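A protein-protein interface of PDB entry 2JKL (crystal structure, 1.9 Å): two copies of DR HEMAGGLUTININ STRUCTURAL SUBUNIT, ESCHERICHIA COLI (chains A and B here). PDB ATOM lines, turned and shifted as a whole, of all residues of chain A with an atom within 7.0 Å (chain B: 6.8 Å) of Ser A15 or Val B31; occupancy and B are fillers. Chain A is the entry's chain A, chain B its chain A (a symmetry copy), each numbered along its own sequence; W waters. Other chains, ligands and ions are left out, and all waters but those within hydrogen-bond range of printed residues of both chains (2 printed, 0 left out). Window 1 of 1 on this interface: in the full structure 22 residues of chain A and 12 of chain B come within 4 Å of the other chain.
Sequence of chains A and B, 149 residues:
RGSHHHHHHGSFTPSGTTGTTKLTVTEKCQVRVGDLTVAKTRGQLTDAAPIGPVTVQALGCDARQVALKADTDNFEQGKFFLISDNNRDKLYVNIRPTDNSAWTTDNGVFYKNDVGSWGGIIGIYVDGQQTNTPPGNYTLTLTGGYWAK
The side-chain hydroxyl of Ser A15 is in hydrogen-bond range of the backbone NH of Glu B27 (2.9 Å). OG of Ser A15 sits at hydrogen-bond distance from O of Cys B29, at 2.5 Å. The backbone NH (N) of Val B31 is in hydrogen-bond range of the backbone carbonyl oxygen (O) of Ser A15, 2.9 Å away. The backbone NH (N) of Thr A17 lies within hydrogen-bond range of the backbone carbonyl oxygen (O) of Val B31, at 3.0 Å. OG1 of Thr A17 lies within hydrogen-bond range of N of Val B33. The backbone carbonyl oxygen of Gln A57 sits at hydrogen-bond distance from the backbone NH of Arg B32 (2.9 Å). The backbone carbonyl oxygen (O) of Leu A59 is in hydrogen-bond range of the backbone NH (N) of Gln B30 (2.9 Å). The side-chain sulfur (SG) of Cys A61 forms a disulfide with the side-chain sulfur (SG) of Cys B29. The backbone NH (N) of Gln B30 lies within hydrogen-bond range of the side-chain sulfur (SG) of Cys A61 (3.6 Å). OE2 of Glu B27 sits close to OH of Tyr A146 (3.5 Å). The backbone carbonyl oxygen (O) of Val B33 lies close to the backbone carbonyl oxygen (O) of Thr A18, 3.4 Å away. O of Lys B28 lies close to O of Leu A59.
N of Thr A13 lies within hydrogen-bond range of O of Tyr A146 (2.8 Å). O of Gly A144 lies within hydrogen-bond range of N of Gly A16 (3.4 Å). O of Thr A17 lies within hydrogen-bond range of N of Gly A144, 3.0 Å away. The backbone carbonyl oxygen (O) of Trp A118 lies within hydrogen-bond range of the backbone NH (N) of Ala A58, 3.0 Å away. NE2 of Gln B30 sits at hydrogen-bond distance from OG1 of Thr B26. OE1 of Gln B30 lies within hydrogen-bond range of NE of Arg B32, 2.9 Å away.
Pro A14 touches Pro B135 (O to CB, 3.9 Å). CB of Thr B26 touches OG of Ser A15 (3.6 Å). Gly A16 touches Val B31. Val A56 touches Val B31 (CG1 to CG1, 3.8 Å). Val A56 touches Arg B32 (CA to O, 3.4 Å). Gln A57 touches Val B31 (O to C, 3.9 Å). Ala A58 touches Gln B30 (CA to O, 3.3 Å). Cys B29 touches Leu A59. Arg B32 touches Leu A59 (NE to CD1, 3.8 Å). Gly A145 touches Val B31.
Printed residues of chain B within 4 Å of Ser A15: Thr B26, Glu B27, Cys B29, Gln B30 and Val B31. Gln A65 touches none of the printed residues of chain B. Of the printed residues of chain A, Thr B26 touches Ser A15 (3.6 Å) and Gly A16 (3.6 Å). Of the printed residues of chain A, Lys B28 touches Leu A59. Of the printed residues of chain A, Val B31 touches Ser A15, Gly A16, Thr A17, Val A56, Gln A57, Gly A144 and Gly A145. The nearest residue of chain B that does not touch Ser A15 is Lys B28 (5.0 Å).
No position is printed for both chains. Of the 34 pairs that touch across the chains among the printed residues, none has its exchanged pair printed and touching as well.
Water W1 bridges the backbone carbonyl oxygen (O) of Val B33 (2.8 Å) and the backbone carbonyl oxygen (O) of Thr A18 (2.9 Å). Water W2 lies within hydrogen-bond range of O of Arg B32 (2.9 Å) and OG1 of Thr A55 (3.1 Å).
Printed residues of chain B that touch a printed residue of chain A: Thr B24, Thr B26, Glu B27, Lys B28, Cys B29, Gln B30, Val B31, Arg B32, Val B33 and Pro B135. Printed residues of chain A that touch a printed residue of chain B: Thr A13, Pro A14, Ser A15, Gly A16, Thr A17, Thr A18, Thr A55, Val A56, Gln A57, Ala A58, Leu A59, Cys A61, Leu A68, Gly A144, Gly A145 and Tyr A146. Hydrophobic or aromatic side chains of chain A that line the printed part of chain B: Val A56, Ala A58, Leu A59, Leu A68 and Tyr A146. Along chain A the printed residues that touch a printed residue of chain B span positions 13 to 146.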
ATOM      1  N   PHE A  12      -1.222   4.114 -19.552  1.00  0.00           N
ATOM      2  CA  PHE A  12      -1.190   2.704 -19.169  1.00  0.00           C
ATOM      3  C   PHE A  12      -0.360   1.893 -20.157  1.00  0.00           C
ATOM      4  O   PHE A  12      -0.525   2.018 -21.371  1.00  0.00           O
ATOM      5  CB  PHE A  12      -2.610   2.128 -19.114  1.00  0.00           C
ATOM      6  CG  PHE A  12      -2.656   0.635 -18.907  1.00  0.00           C
ATOM      7  CD1 PHE A  12      -2.858  -0.226 -19.980  1.00  0.00           C
ATOM      8  CD2 PHE A  12      -2.534   0.092 -17.633  1.00  0.00           C
ATOM      9  CE1 PHE A  12      -2.935  -1.602 -19.784  1.00  0.00           C
ATOM     10  CE2 PHE A  12      -2.596  -1.284 -17.437  1.00  0.00           C
ATOM     11  CZ  PHE A  12      -2.804  -2.129 -18.515  1.00  0.00           C
ATOM     12  N   THR A  13       0.524   1.058 -19.623  1.00  0.00           N
ATOM     13  CA  THR A  13       1.353   0.176 -20.433  1.00  0.00           C
ATOM     14  C   THR A  13       0.908  -1.278 -20.204  1.00  0.00           C
ATOM     15  O   THR A  13       1.127  -1.828 -19.123  1.00  0.00           O
ATOM     16  CB  THR A  13       2.851   0.325 -20.070  1.00  0.00           C
ATOM     17  OG1 THR A  13       3.300   1.658 -20.347  1.00  0.00           O
ATOM     18  CG2 THR A  13       3.686  -0.657 -20.871  1.00  0.00           C
ATOM     19  N   PRO A  14       0.310  -1.904 -21.218  1.00  0.00           N
ATOM     20  CA  PRO A  14      -0.105  -3.300 -21.094  1.00  0.00           C
ATOM     21  C   PRO A  14       1.132  -4.157 -20.820  1.00  0.00           C
ATOM     22  O   PRO A  14       2.110  -4.103 -21.566  1.00  0.00           O
ATOM     23  CB  PRO A  14      -0.669  -3.627 -22.485  1.00  0.00           C
ATOM     24  CG  PRO A  14      -1.056  -2.315 -23.062  1.00  0.00           C
ATOM     25  CD  PRO A  14      -0.082  -1.319 -22.513  1.00  0.00           C
ATOM     26  N   SER A  15       1.098  -4.918 -19.732  1.00  0.00           N
ATOM     27  CA  SER A  15       2.212  -5.787 -19.377  1.00  0.00           C
ATOM     28  C   SER A  15       1.747  -6.777 -18.324  1.00  0.00           C
ATOM     29  O   SER A  15       1.893  -6.540 -17.130  1.00  0.00           O
ATOM     30  CB  SER A  15       3.409  -4.979 -18.856  1.00  0.00           C
ATOM     31  OG  SER A  15       4.505  -5.836 -18.566  1.00  0.00           O
ATOM     32  N   GLY A  16       1.134  -7.864 -18.781  1.00  0.00           N
ATOM     33  CA  GLY A  16       0.611  -8.865 -17.874  1.00  0.00           C
ATOM     34  C   GLY A  16      -0.467  -9.682 -18.567  1.00  0.00           C
ATOM     35  O   GLY A  16      -0.631  -9.613 -19.789  1.00  0.00           O
ATOM     36  N   THR A  17      -1.200 -10.454 -17.775  1.00  0.00           N
ATOM     37  CA  THR A  17      -2.244 -11.313 -18.305  1.00  0.00           C
ATOM     38  C   THR A  17      -3.625 -10.693 -18.127  1.00  0.00           C
ATOM     39  O   THR A  17      -3.773  -9.627 -17.533  1.00  0.00           O
ATOM     40  CB  THR A  17      -2.166 -12.715 -17.695  1.00  0.00           C
ATOM     41  OG1 THR A  17      -2.367 -12.626 -16.276  1.00  0.00           O
ATOM     42  CG2 THR A  17      -0.791 -13.342 -17.981  1.00  0.00           C
ATOM     43  N   THR A  18      -4.635 -11.386 -18.637  1.00  0.00           N
ATOM     44  CA  THR A  18      -6.005 -10.899 -18.595  1.00  0.00           C
ATOM     45  C   THR A  18      -6.900 -11.781 -17.737  1.00  0.00           C
ATOM     46  O   THR A  18      -6.871 -13.010 -17.841  1.00  0.00           O
ATOM     47  CB  THR A  18      -6.569 -10.767 -20.022  1.00  0.00           C
ATOM     48  OG1 THR A  18      -5.739  -9.879 -20.779  1.00  0.00           O
ATOM     49  CG2 THR A  18      -8.000 -10.228 -20.003  1.00  0.00           C
ATOM     50  N   THR A  55      -7.858 -12.163  -8.814  1.00  0.00           N
ATOM     51  CA  THR A  55      -6.524 -12.204  -8.219  1.00  0.00           C
ATOM     52  C   THR A  55      -5.550 -11.354  -9.017  1.00  0.00           C
ATOM     53  O   THR A  55      -5.643 -11.268 -10.248  1.00  0.00           O
ATOM     54  CB  THR A  55      -5.987 -13.633  -8.087  1.00  0.00           C
ATOM     55  OG1 THR A  55      -5.904 -14.230  -9.391  1.00  0.00           O
ATOM     56  CG2 THR A  55      -6.880 -14.474  -7.172  1.00  0.00           C
ATOM     57  N   VAL A  56      -4.600 -10.749  -8.309  1.00  0.00           N
ATOM     58  CA  VAL A  56      -3.571  -9.942  -8.940  1.00  0.00           C
ATOM     59  C   VAL A  56      -2.230 -10.282  -8.299  1.00  0.00           C
ATOM     60  O   VAL A  56      -2.094 -10.258  -7.075  1.00  0.00           O
ATOM     61  CB  VAL A  56      -3.861  -8.427  -8.813  1.00  0.00           C
ATOM     62  CG1 VAL A  56      -2.735  -7.624  -9.463  1.00  0.00           C
ATOM     63  CG2 VAL A  56      -5.214  -8.066  -9.430  1.00  0.00           C
ATOM     64  N   GLN A  57      -1.250 -10.615  -9.131  1.00  0.00           N
ATOM     65  CA  GLN A  57       0.093 -10.919  -8.654  1.00  0.00           C
ATOM     66  C   GLN A  57       1.108 -10.220  -9.558  1.00  0.00           C
ATOM     67  O   GLN A  57       1.284 -10.593 -10.714  1.00  0.00           O
ATOM     68  CB  GLN A  57       0.344 -12.433  -8.643  1.00  0.00           C
ATOM     69  CG  GLN A  57      -0.513 -13.193  -7.615  1.00  0.00           C
ATOM     70  CD  GLN A  57       0.033 -13.079  -6.205  1.00  0.00           C
ATOM     71  OE1 GLN A  57       0.939 -12.295  -5.951  1.00  0.00           O
ATOM     72  NE2 GLN A  57      -0.514 -13.869  -5.282  1.00  0.00           N
ATOM     73  N   ALA A  58       1.761  -9.197  -9.025  1.00  0.00           N
ATOM     74  CA  ALA A  58       2.749  -8.440  -9.780  1.00  0.00           C
ATOM     75  C   ALA A  58       4.160  -8.891  -9.437  1.00  0.00           C
ATOM     76  O   ALA A  58       4.441  -9.291  -8.301  1.00  0.00           O
ATOM     77  CB  ALA A  58       2.589  -6.946  -9.513  1.00  0.00           C
ATOM     78  N   LEU A  59       5.036  -8.842 -10.435  1.00  0.00           N
ATOM     79  CA  LEU A  59       6.437  -9.225 -10.277  1.00  0.00           C
ATOM     80  C   LEU A  59       7.287  -8.255 -11.090  1.00  0.00           C
ATOM     81  O   LEU A  59       6.942  -7.926 -12.224  1.00  0.00           O
ATOM     82  CB  LEU A  59       6.685 -10.640 -10.820  1.00  0.00           C
ATOM     83  CG  LEU A  59       5.973 -11.833 -10.180  1.00  0.00           C
ATOM     84  CD1 LEU A  59       4.823 -12.292 -11.047  1.00  0.00           C
ATOM     85  CD2 LEU A  59       6.963 -12.971  -9.950  1.00  0.00           C
ATOM     86  N   CYS A  61       7.867  -5.123 -10.393  1.00  0.00           N
ATOM     87  CA  CYS A  61       7.290  -3.779 -10.385  1.00  0.00           C
ATOM     88  C   CYS A  61       7.688  -2.923  -9.183  1.00  0.00           C
ATOM     89  O   CYS A  61       6.911  -2.093  -8.720  1.00  0.00           O
ATOM     90  CB  CYS A  61       5.764  -3.867 -10.491  1.00  0.00           C
ATOM     91  SG  CYS A  61       5.205  -4.841 -11.920  1.00  0.00           S
ATOM     92  N   GLN A  65       3.822   1.603 -10.847  1.00  0.00           N
ATOM     93  CA  GLN A  65       2.516   1.526 -10.198  1.00  0.00           C
ATOM     94  C   GLN A  65       1.687   0.468 -10.923  1.00  0.00           C
ATOM     95  O   GLN A  65       1.358   0.632 -12.092  1.00  0.00           O
ATOM     96  CB  GLN A  65       1.782   2.871 -10.300  1.00  0.00           C
ATOM     97  CG  GLN A  65       2.310   3.957  -9.372  1.00  0.00           C
ATOM     98  CD  GLN A  65       1.781   5.332  -9.731  1.00  0.00           C
ATOM     99  OE1 GLN A  65       2.400   6.102 -10.422  1.00  0.00           O
ATOM    100  NE2 GLN A  65       0.556   5.622  -9.250  1.00  0.00           N
ATOM    101  N   VAL A  66       1.323  -0.593 -10.210  1.00  0.00           N
ATOM    102  CA  VAL A  66       0.518  -1.675 -10.768  1.00  0.00           C
ATOM    103  C   VAL A  66      -0.831  -1.132 -11.237  1.00  0.00           C
ATOM    104  O   VAL A  66      -1.423  -0.266 -10.585  1.00  0.00           O
ATOM    105  CB  VAL A  66       0.348  -2.814  -9.734  1.00  0.00           C
ATOM    106  CG1 VAL A  66      -0.799  -3.738 -10.121  1.00  0.00           C
ATOM    107  CG2 VAL A  66       1.649  -3.591  -9.588  1.00  0.00           C
ATOM    108  N   ALA A  67      -1.313  -1.643 -12.366  1.00  0.00           N
ATOM    109  CA  ALA A  67      -2.584  -1.187 -12.928  1.00  0.00           C
ATOM    110  C   ALA A  67      -3.362  -2.291 -13.647  1.00  0.00           C
ATOM    111  O   ALA A  67      -2.793  -3.291 -14.092  1.00  0.00           O
ATOM    112  CB  ALA A  67      -2.350  -0.004 -13.884  1.00  0.00           C
ATOM    113  N   LEU A  68      -4.670  -2.081 -13.759  1.00  0.00           N
ATOM    114  CA  LEU A  68      -5.561  -2.980 -14.475  1.00  0.00           C
ATOM    115  C   LEU A  68      -6.351  -2.090 -15.416  1.00  0.00           C
ATOM    116  O   LEU A  68      -6.856  -1.054 -14.999  1.00  0.00           O
ATOM    117  CB  LEU A  68      -6.547  -3.662 -13.517  1.00  0.00           C
ATOM    118  CG  LEU A  68      -5.989  -4.592 -12.435  1.00  0.00           C
ATOM    119  CD1 LEU A  68      -5.309  -5.798 -13.046  1.00  0.00           C
ATOM    120  CD2 LEU A  68      -5.031  -3.847 -11.516  1.00  0.00           C
ATOM    121  N   TRP A 118       2.776  -5.305  -6.009  1.00  0.00           N
ATOM    122  CA  TRP A 118       1.606  -5.697  -5.237  1.00  0.00           C
ATOM    123  C   TRP A 118       1.004  -7.039  -5.654  1.00  0.00           C
ATOM    124  O   TRP A 118       0.928  -7.374  -6.838  1.00  0.00           O
ATOM    125  CB  TRP A 118       0.535  -4.609  -5.366  1.00  0.00           C
ATOM    126  CG  TRP A 118      -0.678  -4.792  -4.479  1.00  0.00           C
ATOM    127  CD1 TRP A 118      -0.753  -4.546  -3.131  1.00  0.00           C
ATOM    128  CD2 TRP A 118      -2.007  -5.162  -4.893  1.00  0.00           C
ATOM    129  NE1 TRP A 118      -2.035  -4.759  -2.684  1.00  0.00           N
ATOM    130  CE2 TRP A 118      -2.823  -5.140  -3.742  1.00  0.00           C
ATOM    131  CE3 TRP A 118      -2.581  -5.512  -6.122  1.00  0.00           C
ATOM    132  CZ2 TRP A 118      -4.182  -5.453  -3.783  1.00  0.00           C
ATOM    133  CZ3 TRP A 118      -3.926  -5.847  -6.156  1.00  0.00           C
ATOM    134  CH2 TRP A 118      -4.712  -5.816  -4.990  1.00  0.00           C
ATOM    135  N   THR A 143      -7.057  -6.219 -17.974  1.00  0.00           N
ATOM    136  CA  THR A 143      -5.690  -6.561 -18.379  1.00  0.00           C
ATOM    137  C   THR A 143      -4.665  -5.922 -17.442  1.00  0.00           C
ATOM    138  O   THR A 143      -4.773  -4.741 -17.106  1.00  0.00           O
ATOM    139  CB  THR A 143      -5.434  -6.121 -19.836  1.00  0.00           C
ATOM    140  OG1 THR A 143      -6.348  -6.796 -20.707  1.00  0.00           O
ATOM    141  CG2 THR A 143      -4.005  -6.442 -20.261  1.00  0.00           C
ATOM    142  N   GLY A 144      -3.654  -6.697 -17.053  1.00  0.00           N
ATOM    143  CA  GLY A 144      -2.617  -6.206 -16.144  1.00  0.00           C
ATOM    144  C   GLY A 144      -1.552  -5.380 -16.858  1.00  0.00           C
ATOM    145  O   GLY A 144      -1.238  -5.617 -18.024  1.00  0.00           O
ATOM    146  N   GLY A 145      -0.980  -4.422 -16.139  1.00  0.00           N
ATOM    147  CA  GLY A 145       0.073  -3.579 -16.692  1.00  0.00           C
ATOM    148  C   GLY A 145       0.499  -2.575 -15.635  1.00  0.00           C
ATOM    149  O   GLY A 145       0.324  -2.807 -14.442  1.00  0.00           O
ATOM    150  N   TYR A 146       1.039  -1.445 -16.071  1.00  0.00           N
ATOM    151  CA  TYR A 146       1.438  -0.413 -15.123  1.00  0.00           C
ATOM    152  C   TYR A 146       1.099   0.989 -15.628  1.00  0.00           C
ATOM    153  O   TYR A 146       0.936   1.202 -16.829  1.00  0.00           O
ATOM    154  CB  TYR A 146       2.904  -0.553 -14.724  1.00  0.00           C
ATOM    155  CG  TYR A 146       3.876  -0.505 -15.878  1.00  0.00           C
ATOM    156  CD1 TYR A 146       4.338  -1.672 -16.476  1.00  0.00           C
ATOM    157  CD2 TYR A 146       4.384   0.708 -16.325  1.00  0.00           C
ATOM    158  CE1 TYR A 146       5.259  -1.629 -17.504  1.00  0.00           C
ATOM    159  CE2 TYR A 146       5.306   0.762 -17.353  1.00  0.00           C
ATOM    160  CZ  TYR A 146       5.735  -0.409 -17.943  1.00  0.00           C
ATOM    161  OH  TYR A 146       6.648  -0.345 -18.972  1.00  0.00           O
ATOM    162  N   THR B  24       1.796 -15.386 -23.166  1.00  0.00           N
ATOM    163  CA  THR B  24       1.628 -13.954 -22.988  1.00  0.00           C
ATOM    164  C   THR B  24       3.018 -13.371 -22.741  1.00  0.00           C
ATOM    165  O   THR B  24       3.750 -13.833 -21.865  1.00  0.00           O
ATOM    166  CB  THR B  24       0.649 -13.615 -21.841  1.00  0.00           C
ATOM    167  OG1 THR B  24      -0.678 -14.022 -22.206  1.00  0.00           O
ATOM    168  CG2 THR B  24       0.656 -12.111 -21.572  1.00  0.00           C
ATOM    169  N   VAL B  25       3.405 -12.410 -23.571  1.00  0.00           N
ATOM    170  CA  VAL B  25       4.699 -11.750 -23.448  1.00  0.00           C
ATOM    171  C   VAL B  25       4.478 -10.436 -22.704  1.00  0.00           C
ATOM    172  O   VAL B  25       3.518  -9.722 -22.969  1.00  0.00           O
ATOM    173  CB  VAL B  25       5.342 -11.511 -24.830  1.00  0.00           C
ATOM    174  CG1 VAL B  25       6.633 -10.725 -24.681  1.00  0.00           C
ATOM    175  CG2 VAL B  25       5.617 -12.839 -25.530  1.00  0.00           C
ATOM    176  N   THR B  26       5.359 -10.131 -21.759  1.00  0.00           N
ATOM    177  CA  THR B  26       5.221  -8.928 -20.954  1.00  0.00           C
ATOM    178  C   THR B  26       6.573  -8.233 -20.852  1.00  0.00           C
ATOM    179  O   THR B  26       7.571  -8.738 -21.345  1.00  0.00           O
ATOM    180  CB  THR B  26       4.762  -9.293 -19.527  1.00  0.00           C
ATOM    181  OG1 THR B  26       5.880  -9.815 -18.803  1.00  0.00           O
ATOM    182  CG2 THR B  26       3.662 -10.352 -19.557  1.00  0.00           C
ATOM    183  N   GLU B  27       6.598  -7.104 -20.151  1.00  0.00           N
ATOM    184  CA  GLU B  27       7.836  -6.400 -19.850  1.00  0.00           C
ATOM    185  C   GLU B  27       8.329  -6.964 -18.514  1.00  0.00           C
ATOM    186  O   GLU B  27       7.722  -7.892 -17.970  1.00  0.00           O
ATOM    187  CB  GLU B  27       7.565  -4.901 -19.695  1.00  0.00           C
ATOM    188  CG  GLU B  27       7.045  -4.230 -20.958  1.00  0.00           C
ATOM    189  CD  GLU B  27       7.255  -2.732 -20.938  1.00  0.00           C
ATOM    190  OE1 GLU B  27       7.663  -2.209 -19.878  1.00  0.00           O
ATOM    191  OE2 GLU B  27       7.012  -2.080 -21.977  1.00  0.00           O
ATOM    192  N   LYS B  28       9.411  -6.396 -17.983  1.00  0.00           N
ATOM    193  CA  LYS B  28       9.956  -6.825 -16.697  1.00  0.00           C
ATOM    194  C   LYS B  28       8.914  -6.680 -15.587  1.00  0.00           C
ATOM    195  O   LYS B  28       8.755  -7.580 -14.756  1.00  0.00           O
ATOM    196  CB  LYS B  28      11.223  -6.029 -16.354  1.00  0.00           C
ATOM    197  CG  LYS B  28      11.827  -6.384 -15.003  1.00  0.00           C
ATOM    198  CD  LYS B  28      12.604  -5.214 -14.417  1.00  0.00           C
ATOM    199  CE  LYS B  28      12.074  -4.829 -13.043  1.00  0.00           C
ATOM    200  NZ  LYS B  28      13.167  -4.676 -12.042  1.00  0.00           N
ATOM    201  N   CYS B  29       8.196  -5.557 -15.582  1.00  0.00           N
ATOM    202  CA  CYS B  29       7.110  -5.354 -14.618  1.00  0.00           C
ATOM    203  C   CYS B  29       5.924  -6.072 -15.241  1.00  0.00           C
ATOM    204  O   CYS B  29       5.404  -5.669 -16.287  1.00  0.00           O
ATOM    205  CB  CYS B  29       6.811  -3.874 -14.383  1.00  0.00           C
ATOM    206  SG  CYS B  29       5.261  -3.532 -13.473  1.00  0.00           S
ATOM    207  N   GLN B  30       5.582  -7.200 -14.630  1.00  0.00           N
ATOM    208  CA  GLN B  30       4.587  -8.130 -15.133  1.00  0.00           C
ATOM    209  C   GLN B  30       3.418  -8.272 -14.153  1.00  0.00           C
ATOM    210  O   GLN B  30       3.616  -8.588 -12.984  1.00  0.00           O
ATOM    211  CB  GLN B  30       5.301  -9.469 -15.298  1.00  0.00           C
ATOM    212  CG  GLN B  30       4.462 -10.662 -15.645  1.00  0.00           C
ATOM    213  CD  GLN B  30       5.311 -11.912 -15.700  1.00  0.00           C
ATOM    214  OE1 GLN B  30       5.492 -12.593 -14.691  1.00  0.00           O
ATOM    215  NE2 GLN B  30       5.949 -12.141 -16.841  1.00  0.00           N
ATOM    216  N   VAL B  31       2.203  -8.026 -14.636  1.00  0.00           N
ATOM    217  CA  VAL B  31       1.019  -8.094 -13.774  1.00  0.00           C
ATOM    218  C   VAL B  31       0.076  -9.231 -14.164  1.00  0.00           C
ATOM    219  O   VAL B  31      -0.658  -9.140 -15.149  1.00  0.00           O
ATOM    220  CB  VAL B  31       0.301  -6.736 -13.695  1.00  0.00           C
ATOM    221  CG1 VAL B  31      -0.889  -6.812 -12.742  1.00  0.00           C
ATOM    222  CG2 VAL B  31       1.277  -5.653 -13.251  1.00  0.00           C
ATOM    223  N   ARG B  32       0.119 -10.309 -13.390  1.00  0.00           N
ATOM    224  CA  ARG B  32      -0.696 -11.485 -13.659  1.00  0.00           C
ATOM    225  C   ARG B  32      -2.081 -11.347 -13.040  1.00  0.00           C
ATOM    226  O   ARG B  32      -2.225 -11.283 -11.818  1.00  0.00           O
ATOM    227  CB  ARG B  32      -0.001 -12.741 -13.126  1.00  0.00           C
ATOM    228  CG  ARG B  32       1.336 -13.002 -13.787  1.00  0.00           C
ATOM    229  CD  ARG B  32       2.046 -14.204 -13.194  1.00  0.00           C
ATOM    230  NE  ARG B  32       3.351 -14.397 -13.825  1.00  0.00           N
ATOM    231  CZ  ARG B  32       3.655 -15.424 -14.609  1.00  0.00           C
ATOM    232  NH1 ARG B  32       2.752 -16.370 -14.854  1.00  0.00           N
ATOM    233  NH2 ARG B  32       4.867 -15.512 -15.143  1.00  0.00           N
ATOM    234  N   VAL B  33      -3.092 -11.334 -13.897  1.00  0.00           N
ATOM    235  CA  VAL B  33      -4.480 -11.182 -13.479  1.00  0.00           C
ATOM    236  C   VAL B  33      -5.270 -12.468 -13.715  1.00  0.00           C
ATOM    237  O   VAL B  33      -5.314 -12.988 -14.828  1.00  0.00           O
ATOM    238  CB  VAL B  33      -5.141 -10.001 -14.228  1.00  0.00           C
ATOM    239  CG1 VAL B  33      -6.557  -9.746 -13.702  1.00  0.00           C
ATOM    240  CG2 VAL B  33      -4.271  -8.747 -14.114  1.00  0.00           C
ATOM    241  N   PRO B 135       4.936  -6.781 -26.147  1.00  0.00           N
ATOM    242  CA  PRO B 135       4.065  -7.456 -25.185  1.00  0.00           C
ATOM    243  C   PRO B 135       2.713  -7.712 -25.836  1.00  0.00           C
ATOM    244  O   PRO B 135       2.235  -6.900 -26.628  1.00  0.00           O
ATOM    245  CB  PRO B 135       3.933  -6.428 -24.063  1.00  0.00           C
ATOM    246  CG  PRO B 135       5.242  -5.713 -24.095  1.00  0.00           C
ATOM    247  CD  PRO B 135       5.565  -5.584 -25.560  1.00  0.00           C
HETATM  248  O   HOH W   1      -5.732 -15.283 -16.380  1.00  0.00           O
HETATM  249  O   HOH W   2      -3.135 -13.749 -10.716  1.00  0.00           O
